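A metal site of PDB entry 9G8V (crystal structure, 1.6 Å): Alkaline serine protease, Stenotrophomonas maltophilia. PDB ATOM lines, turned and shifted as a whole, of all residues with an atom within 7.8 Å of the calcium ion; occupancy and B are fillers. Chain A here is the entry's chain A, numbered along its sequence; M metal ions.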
ATOM      1  N   PRO A   3      -9.680  13.468 -30.309  1.00  0.00           N
ATOM      2  CA  PRO A   3      -8.473  13.140 -29.540  1.00  0.00           C
ATOM      3  C   PRO A   3      -7.809  11.859 -30.050  1.00  0.00           C
ATOM      4  O   PRO A   3      -8.455  11.040 -30.710  1.00  0.00           O
ATOM      5  CB  PRO A   3      -9.019  12.978 -28.111  1.00  0.00           C
ATOM      6  CG  PRO A   3     -10.423  12.470 -28.367  1.00  0.00           C
ATOM      7  CD  PRO A   3     -10.936  13.321 -29.534  1.00  0.00           C
ATOM      8  N   ASN A   4      -6.527  11.692 -29.677  1.00  0.00           N
ATOM      9  CA  ASN A   4      -5.732  10.623 -30.299  1.00  0.00           C
ATOM     10  C   ASN A   4      -5.750   9.331 -29.451  1.00  0.00           C
ATOM     11  O   ASN A   4      -4.993   8.400 -29.739  1.00  0.00           O
ATOM     12  CB  ASN A   4      -4.289  11.080 -30.517  1.00  0.00           C
ATOM     13  CG  ASN A   4      -3.560  11.305 -29.210  1.00  0.00           C
ATOM     14  OD1 ASN A   4      -4.115  11.095 -28.137  1.00  0.00           O
ATOM     15  ND2 ASN A   4      -2.318  11.779 -29.261  1.00  0.00           N
ATOM     16  N   ASP A   5      -6.593   9.256 -28.414  1.00  0.00           N
ATOM     17  CA  ASP A   5      -6.585   8.051 -27.577  1.00  0.00           C
ATOM     18  C   ASP A   5      -6.853   6.838 -28.444  1.00  0.00           C
ATOM     19  O   ASP A   5      -7.851   6.810 -29.166  1.00  0.00           O
ATOM     20  CB  ASP A   5      -7.558   8.152 -26.422  1.00  0.00           C
ATOM     21  CG  ASP A   5      -7.391   9.463 -25.661  1.00  0.00           C
ATOM     22  OD1 ASP A   5      -7.851  10.512 -26.194  1.00  0.00           O
ATOM     23  OD2 ASP A   5      -6.711   9.469 -24.612  1.00  0.00           O
ATOM     24  N   PRO A   6      -6.007   5.768 -28.391  1.00  0.00           N
ATOM     25  CA  PRO A   6      -6.107   4.666 -29.351  1.00  0.00           C
ATOM     26  C   PRO A   6      -7.442   3.942 -29.396  1.00  0.00           C
ATOM     27  O   PRO A   6      -7.816   3.443 -30.456  1.00  0.00           O
ATOM     28  CB  PRO A   6      -4.940   3.699 -29.045  1.00  0.00           C
ATOM     29  CG  PRO A   6      -4.426   4.179 -27.684  1.00  0.00           C
ATOM     30  CD  PRO A   6      -4.831   5.656 -27.490  1.00  0.00           C
ATOM     31  N   TYR A   7      -8.129   3.811 -28.252  1.00  0.00           N
ATOM     32  CA  TYR A   7      -9.372   3.073 -28.290  1.00  0.00           C
ATOM     33  C   TYR A   7     -10.604   3.979 -28.433  1.00  0.00           C
ATOM     34  O   TYR A   7     -11.729   3.466 -28.447  1.00  0.00           O
ATOM     35  CB  TYR A   7      -9.475   2.265 -26.996  1.00  0.00           C
ATOM     36  CG  TYR A   7      -8.445   1.155 -26.865  1.00  0.00           C
ATOM     37  CD1 TYR A   7      -8.038   0.422 -27.985  1.00  0.00           C
ATOM     38  CD2 TYR A   7      -7.964   0.781 -25.620  1.00  0.00           C
ATOM     39  CE1 TYR A   7      -7.103  -0.604 -27.868  1.00  0.00           C
ATOM     40  CE2 TYR A   7      -7.071  -0.274 -25.490  1.00  0.00           C
ATOM     41  CZ  TYR A   7      -6.643  -0.961 -26.612  1.00  0.00           C
ATOM     42  OH  TYR A   7      -5.762  -2.007 -26.448  1.00  0.00           O
ATOM     43  N   TYR A   8     -10.418   5.300 -28.558  1.00  0.00           N
ATOM     44  CA  TYR A   8     -11.568   6.207 -28.534  1.00  0.00           C
ATOM     45  C   TYR A   8     -12.517   6.016 -29.740  1.00  0.00           C
ATOM     46  O   TYR A   8     -13.737   5.913 -29.576  1.00  0.00           O
ATOM     47  CB  TYR A   8     -11.026   7.636 -28.492  1.00  0.00           C
ATOM     48  CG  TYR A   8     -11.984   8.757 -28.929  1.00  0.00           C
ATOM     49  CD1 TYR A   8     -12.978   9.216 -28.085  1.00  0.00           C
ATOM     50  CD2 TYR A   8     -11.918   9.310 -30.211  1.00  0.00           C
ATOM     51  CE1 TYR A   8     -13.803  10.285 -28.443  1.00  0.00           C
ATOM     52  CE2 TYR A   8     -12.722  10.372 -30.591  1.00  0.00           C
ATOM     53  CZ  TYR A   8     -13.714  10.816 -29.720  1.00  0.00           C
ATOM     54  OH  TYR A   8     -14.545  11.831 -30.085  1.00  0.00           O
ATOM     55  N   GLN A  12     -15.751   4.243 -28.165  1.00  0.00           N
ATOM     56  CA  GLN A  12     -16.423   5.255 -27.327  1.00  0.00           C
ATOM     57  C   GLN A  12     -17.564   6.000 -28.052  1.00  0.00           C
ATOM     58  O   GLN A  12     -17.651   7.247 -28.045  1.00  0.00           O
ATOM     59  CB  GLN A  12     -15.482   6.193 -26.546  1.00  0.00           C
ATOM     60  CG  GLN A  12     -14.680   5.437 -25.490  1.00  0.00           C
ATOM     61  CD  GLN A  12     -13.747   6.343 -24.734  1.00  0.00           C
ATOM     62  OE1 GLN A  12     -12.892   7.033 -25.312  1.00  0.00           O
ATOM     63  NE2 GLN A  12     -14.010   6.459 -23.441  1.00  0.00           N
ATOM     64  N   PRO A  50      -2.718   4.480 -15.251  1.00  0.00           N
ATOM     65  CA  PRO A  50      -1.918   5.384 -16.065  1.00  0.00           C
ATOM     66  C   PRO A  50      -2.746   6.339 -16.922  1.00  0.00           C
ATOM     67  O   PRO A  50      -2.201   7.352 -17.381  1.00  0.00           O
ATOM     68  CB  PRO A  50      -1.095   4.434 -16.952  1.00  0.00           C
ATOM     69  CG  PRO A  50      -1.921   3.141 -16.964  1.00  0.00           C
ATOM     70  CD  PRO A  50      -2.462   3.060 -15.539  1.00  0.00           C
ATOM     71  N   ASP A  51      -4.048   6.034 -17.082  1.00  0.00           N
ATOM     72  CA  ASP A  51      -4.857   6.966 -17.880  1.00  0.00           C
ATOM     73  C   ASP A  51      -5.706   7.876 -16.971  1.00  0.00           C
ATOM     74  O   ASP A  51      -6.557   8.614 -17.504  1.00  0.00           O
ATOM     75  CB  ASP A  51      -5.766   6.241 -18.862  1.00  0.00           C
ATOM     76  CG  ASP A  51      -5.968   6.975 -20.181  1.00  0.00           C
ATOM     77  OD1 ASP A  51      -5.092   7.812 -20.516  1.00  0.00           O
ATOM     78  OD2 ASP A  51      -7.013   6.751 -20.822  1.00  0.00           O
ATOM     79  N   LEU A  52      -5.502   7.811 -15.637  1.00  0.00           N
ATOM     80  CA  LEU A  52      -6.158   8.718 -14.695  1.00  0.00           C
ATOM     81  C   LEU A  52      -5.176   9.641 -13.956  1.00  0.00           C
ATOM     82  O   LEU A  52      -5.551  10.763 -13.614  1.00  0.00           O
ATOM     83  CB  LEU A  52      -6.944   7.902 -13.653  1.00  0.00           C
ATOM     84  CG  LEU A  52      -8.121   7.079 -14.204  1.00  0.00           C
ATOM     85  CD1 LEU A  52      -8.792   6.441 -12.977  1.00  0.00           C
ATOM     86  CD2 LEU A  52      -9.137   7.900 -14.961  1.00  0.00           C
ATOM     87  N   GLU A 115     -11.191  10.931 -17.445  1.00  0.00           N
ATOM     88  CA  GLU A 115     -10.070  10.148 -17.961  1.00  0.00           C
ATOM     89  C   GLU A 115      -9.167  11.043 -18.826  1.00  0.00           C
ATOM     90  O   GLU A 115      -9.648  11.862 -19.634  1.00  0.00           O
ATOM     91  CB  GLU A 115     -10.605   8.973 -18.782  1.00  0.00           C
ATOM     92  CG  GLU A 115      -9.491   8.034 -19.240  1.00  0.00           C
ATOM     93  CD  GLU A 115      -9.929   6.588 -19.419  1.00  0.00           C
ATOM     94  OE1 GLU A 115     -11.089   6.246 -19.062  1.00  0.00           O
ATOM     95  OE2 GLU A 115      -9.089   5.770 -19.930  1.00  0.00           O
ATOM     96  N   GLN A 116      -7.840  10.905 -18.639  1.00  0.00           N
ATOM     97  CA  GLN A 116      -6.917  11.726 -19.441  1.00  0.00           C
ATOM     98  C   GLN A 116      -7.154  11.473 -20.921  1.00  0.00           C
ATOM     99  O   GLN A 116      -7.220  10.328 -21.393  1.00  0.00           O
ATOM    100  CB  GLN A 116      -5.483  11.333 -19.091  1.00  0.00           C
ATOM    101  CG  GLN A 116      -5.056  11.763 -17.682  1.00  0.00           C
ATOM    102  CD  GLN A 116      -4.531  13.193 -17.681  1.00  0.00           C
ATOM    103  OE1 GLN A 116      -4.853  14.004 -18.544  1.00  0.00           O
ATOM    104  NE2 GLN A 116      -3.700  13.550 -16.706  1.00  0.00           N
ATOM    105  N   THR A 117      -7.183  12.575 -21.680  1.00  0.00           N
ATOM    106  CA  THR A 117      -7.594  12.514 -23.066  1.00  0.00           C
ATOM    107  C   THR A 117      -6.555  13.194 -23.963  1.00  0.00           C
ATOM    108  O   THR A 117      -5.826  14.082 -23.513  1.00  0.00           O
ATOM    109  CB  THR A 117      -8.954  13.194 -23.166  1.00  0.00           C
ATOM    110  OG1 THR A 117      -9.894  12.470 -22.381  1.00  0.00           O
ATOM    111  CG2 THR A 117      -9.531  13.242 -24.572  1.00  0.00           C
ATOM    112  N   ASN A 118      -6.502  12.728 -25.219  1.00  0.00           N
ATOM    113  CA  ASN A 118      -5.527  13.209 -26.178  1.00  0.00           C
ATOM    114  C   ASN A 118      -4.120  12.966 -25.666  1.00  0.00           C
ATOM    115  O   ASN A 118      -3.222  13.733 -26.007  1.00  0.00           O
ATOM    116  CB  ASN A 118      -5.817  14.658 -26.590  1.00  0.00           C
ATOM    117  CG  ASN A 118      -5.284  14.976 -27.969  1.00  0.00           C
ATOM    118  OD1 ASN A 118      -5.286  14.137 -28.870  1.00  0.00           O
ATOM    119  ND2 ASN A 118      -4.774  16.178 -28.152  1.00  0.00           N
ATOM    120  N   ASN A 119      -3.911  11.878 -24.874  1.00  0.00           N
ATOM    121  CA  ASN A 119      -2.600  11.584 -24.325  1.00  0.00           C
ATOM    122  C   ASN A 119      -2.030  10.316 -24.962  1.00  0.00           C
ATOM    123  O   ASN A 119      -1.008   9.794 -24.466  1.00  0.00           O
ATOM    124  CB  ASN A 119      -2.586  11.440 -22.794  1.00  0.00           C
ATOM    125  CG  ASN A 119      -3.409  10.273 -22.294  1.00  0.00           C
ATOM    126  OD1 ASN A 119      -4.332   9.787 -22.978  1.00  0.00           O
ATOM    127  ND2 ASN A 119      -3.065   9.791 -21.108  1.00  0.00           N
ATOM    128  N   GLY A 120      -2.599   9.860 -26.075  1.00  0.00           N
ATOM    129  CA  GLY A 120      -2.012   8.688 -26.743  1.00  0.00           C
ATOM    130  C   GLY A 120      -2.123   7.398 -25.919  1.00  0.00           C
ATOM    131  O   GLY A 120      -1.392   6.444 -26.186  1.00  0.00           O
ATOM    132  N   VAL A 121      -3.041   7.338 -24.944  1.00  0.00           N
ATOM    133  CA  VAL A 121      -3.168   6.153 -24.104  1.00  0.00           C
ATOM    134  C   VAL A 121      -4.643   5.809 -23.904  1.00  0.00           C
ATOM    135  O   VAL A 121      -5.447   6.696 -23.587  1.00  0.00           O
ATOM    136  CB  VAL A 121      -2.521   6.428 -22.731  1.00  0.00           C
ATOM    137  CG1 VAL A 121      -2.733   5.226 -21.806  1.00  0.00           C
ATOM    138  CG2 VAL A 121      -1.028   6.679 -22.813  1.00  0.00           C
ATOM    139  N   GLY A 122      -5.004   4.550 -24.156  1.00  0.00           N
ATOM    140  CA  GLY A 122      -6.320   4.059 -23.728  1.00  0.00           C
ATOM    141  C   GLY A 122      -7.516   4.828 -24.324  1.00  0.00           C
ATOM    142  O   GLY A 122      -7.677   4.887 -25.549  1.00  0.00           O
ATOM    143  N   MET A 123      -8.352   5.372 -23.416  1.00  0.00           N
ATOM    144  CA  MET A 123      -9.642   5.935 -23.788  1.00  0.00           C
ATOM    145  C   MET A 123      -9.680   7.443 -23.494  1.00  0.00           C
ATOM    146  O   MET A 123      -8.744   8.001 -22.912  1.00  0.00           O
ATOM    147  CB  MET A 123     -10.749   5.270 -22.941  1.00  0.00           C
ATOM    148  CG  MET A 123     -10.853   3.738 -23.034  1.00  0.00           C
ATOM    149  SD  MET A 123     -11.814   3.302 -24.478  1.00  0.00           S
ATOM    150  CE  MET A 123     -11.646   1.479 -24.411  1.00  0.00           C
ATOM    151  N   ALA A 124     -10.795   8.102 -23.866  1.00  0.00           N
ATOM    152  CA  ALA A 124     -11.032   9.513 -23.505  1.00  0.00           C
ATOM    153  C   ALA A 124     -12.033   9.621 -22.340  1.00  0.00           C
ATOM    154  O   ALA A 124     -12.709   8.654 -22.021  1.00  0.00           O
ATOM    155  CB  ALA A 124     -11.588  10.195 -24.734  1.00  0.00           C
ATOM    156  N   GLY A 125     -12.101  10.817 -21.733  1.00  0.00           N
ATOM    157  CA  GLY A 125     -13.073  11.174 -20.694  1.00  0.00           C
ATOM    158  C   GLY A 125     -13.740  12.512 -21.070  1.00  0.00           C
ATOM    159  O   GLY A 125     -13.237  13.291 -21.893  1.00  0.00           O
ATOM    160  N   TYR A 282      -8.949  -1.497 -19.618  1.00  0.00           N
ATOM    161  CA  TYR A 282     -10.099  -0.675 -20.038  1.00  0.00           C
ATOM    162  C   TYR A 282     -11.290  -1.629 -20.102  1.00  0.00           C
ATOM    163  O   TYR A 282     -11.167  -2.748 -20.593  1.00  0.00           O
ATOM    164  CB  TYR A 282      -9.825   0.062 -21.343  1.00  0.00           C
ATOM    165  CG  TYR A 282      -8.551   0.883 -21.234  1.00  0.00           C
ATOM    166  CD1 TYR A 282      -8.593   2.160 -20.645  1.00  0.00           C
ATOM    167  CD2 TYR A 282      -7.319   0.373 -21.608  1.00  0.00           C
ATOM    168  CE1 TYR A 282      -7.467   2.910 -20.453  1.00  0.00           C
ATOM    169  CE2 TYR A 282      -6.162   1.105 -21.375  1.00  0.00           C
ATOM    170  CZ  TYR A 282      -6.231   2.364 -20.783  1.00  0.00           C
ATOM    171  OH  TYR A 282      -5.113   3.079 -20.599  1.00  0.00           O
HETATM  172 CA    CA M   1      -6.429   8.505 -22.592  1.00  0.00          CA
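The backbone NH (N) of Asn 118 sits at hydrogen-bond distance from the side-chain carboxylate (OD1) of Asp 5 (2.8 Å). The backbone NH of Asn 119 sits at hydrogen-bond distance from the side-chain amide oxygen of Asn 4. OE2 of Glu 115 sits close to OD2 of Asp 51, at 2.5 Å.
Of the 22 residues printed, 6 come within 4 Å of the calcium ion.
The side-chain carboxylate (OD2) of Asp 5 binds the calcium ion. The calcium ion is bound by O of Val 121 (2.3 Å). O of Gln 116 binds the calcium ion, at 2.3 Å. The calcium ion is bound by O of Met 123. OD1 of Asn 119 binds the calcium ion, 2.5 Å away. The side-chain carboxylate (OD2) of Asp 51 binds the calcium ion, 2.6 Å away. OD1 of Asp 51 binds the calcium ion, at 2.6 Å.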
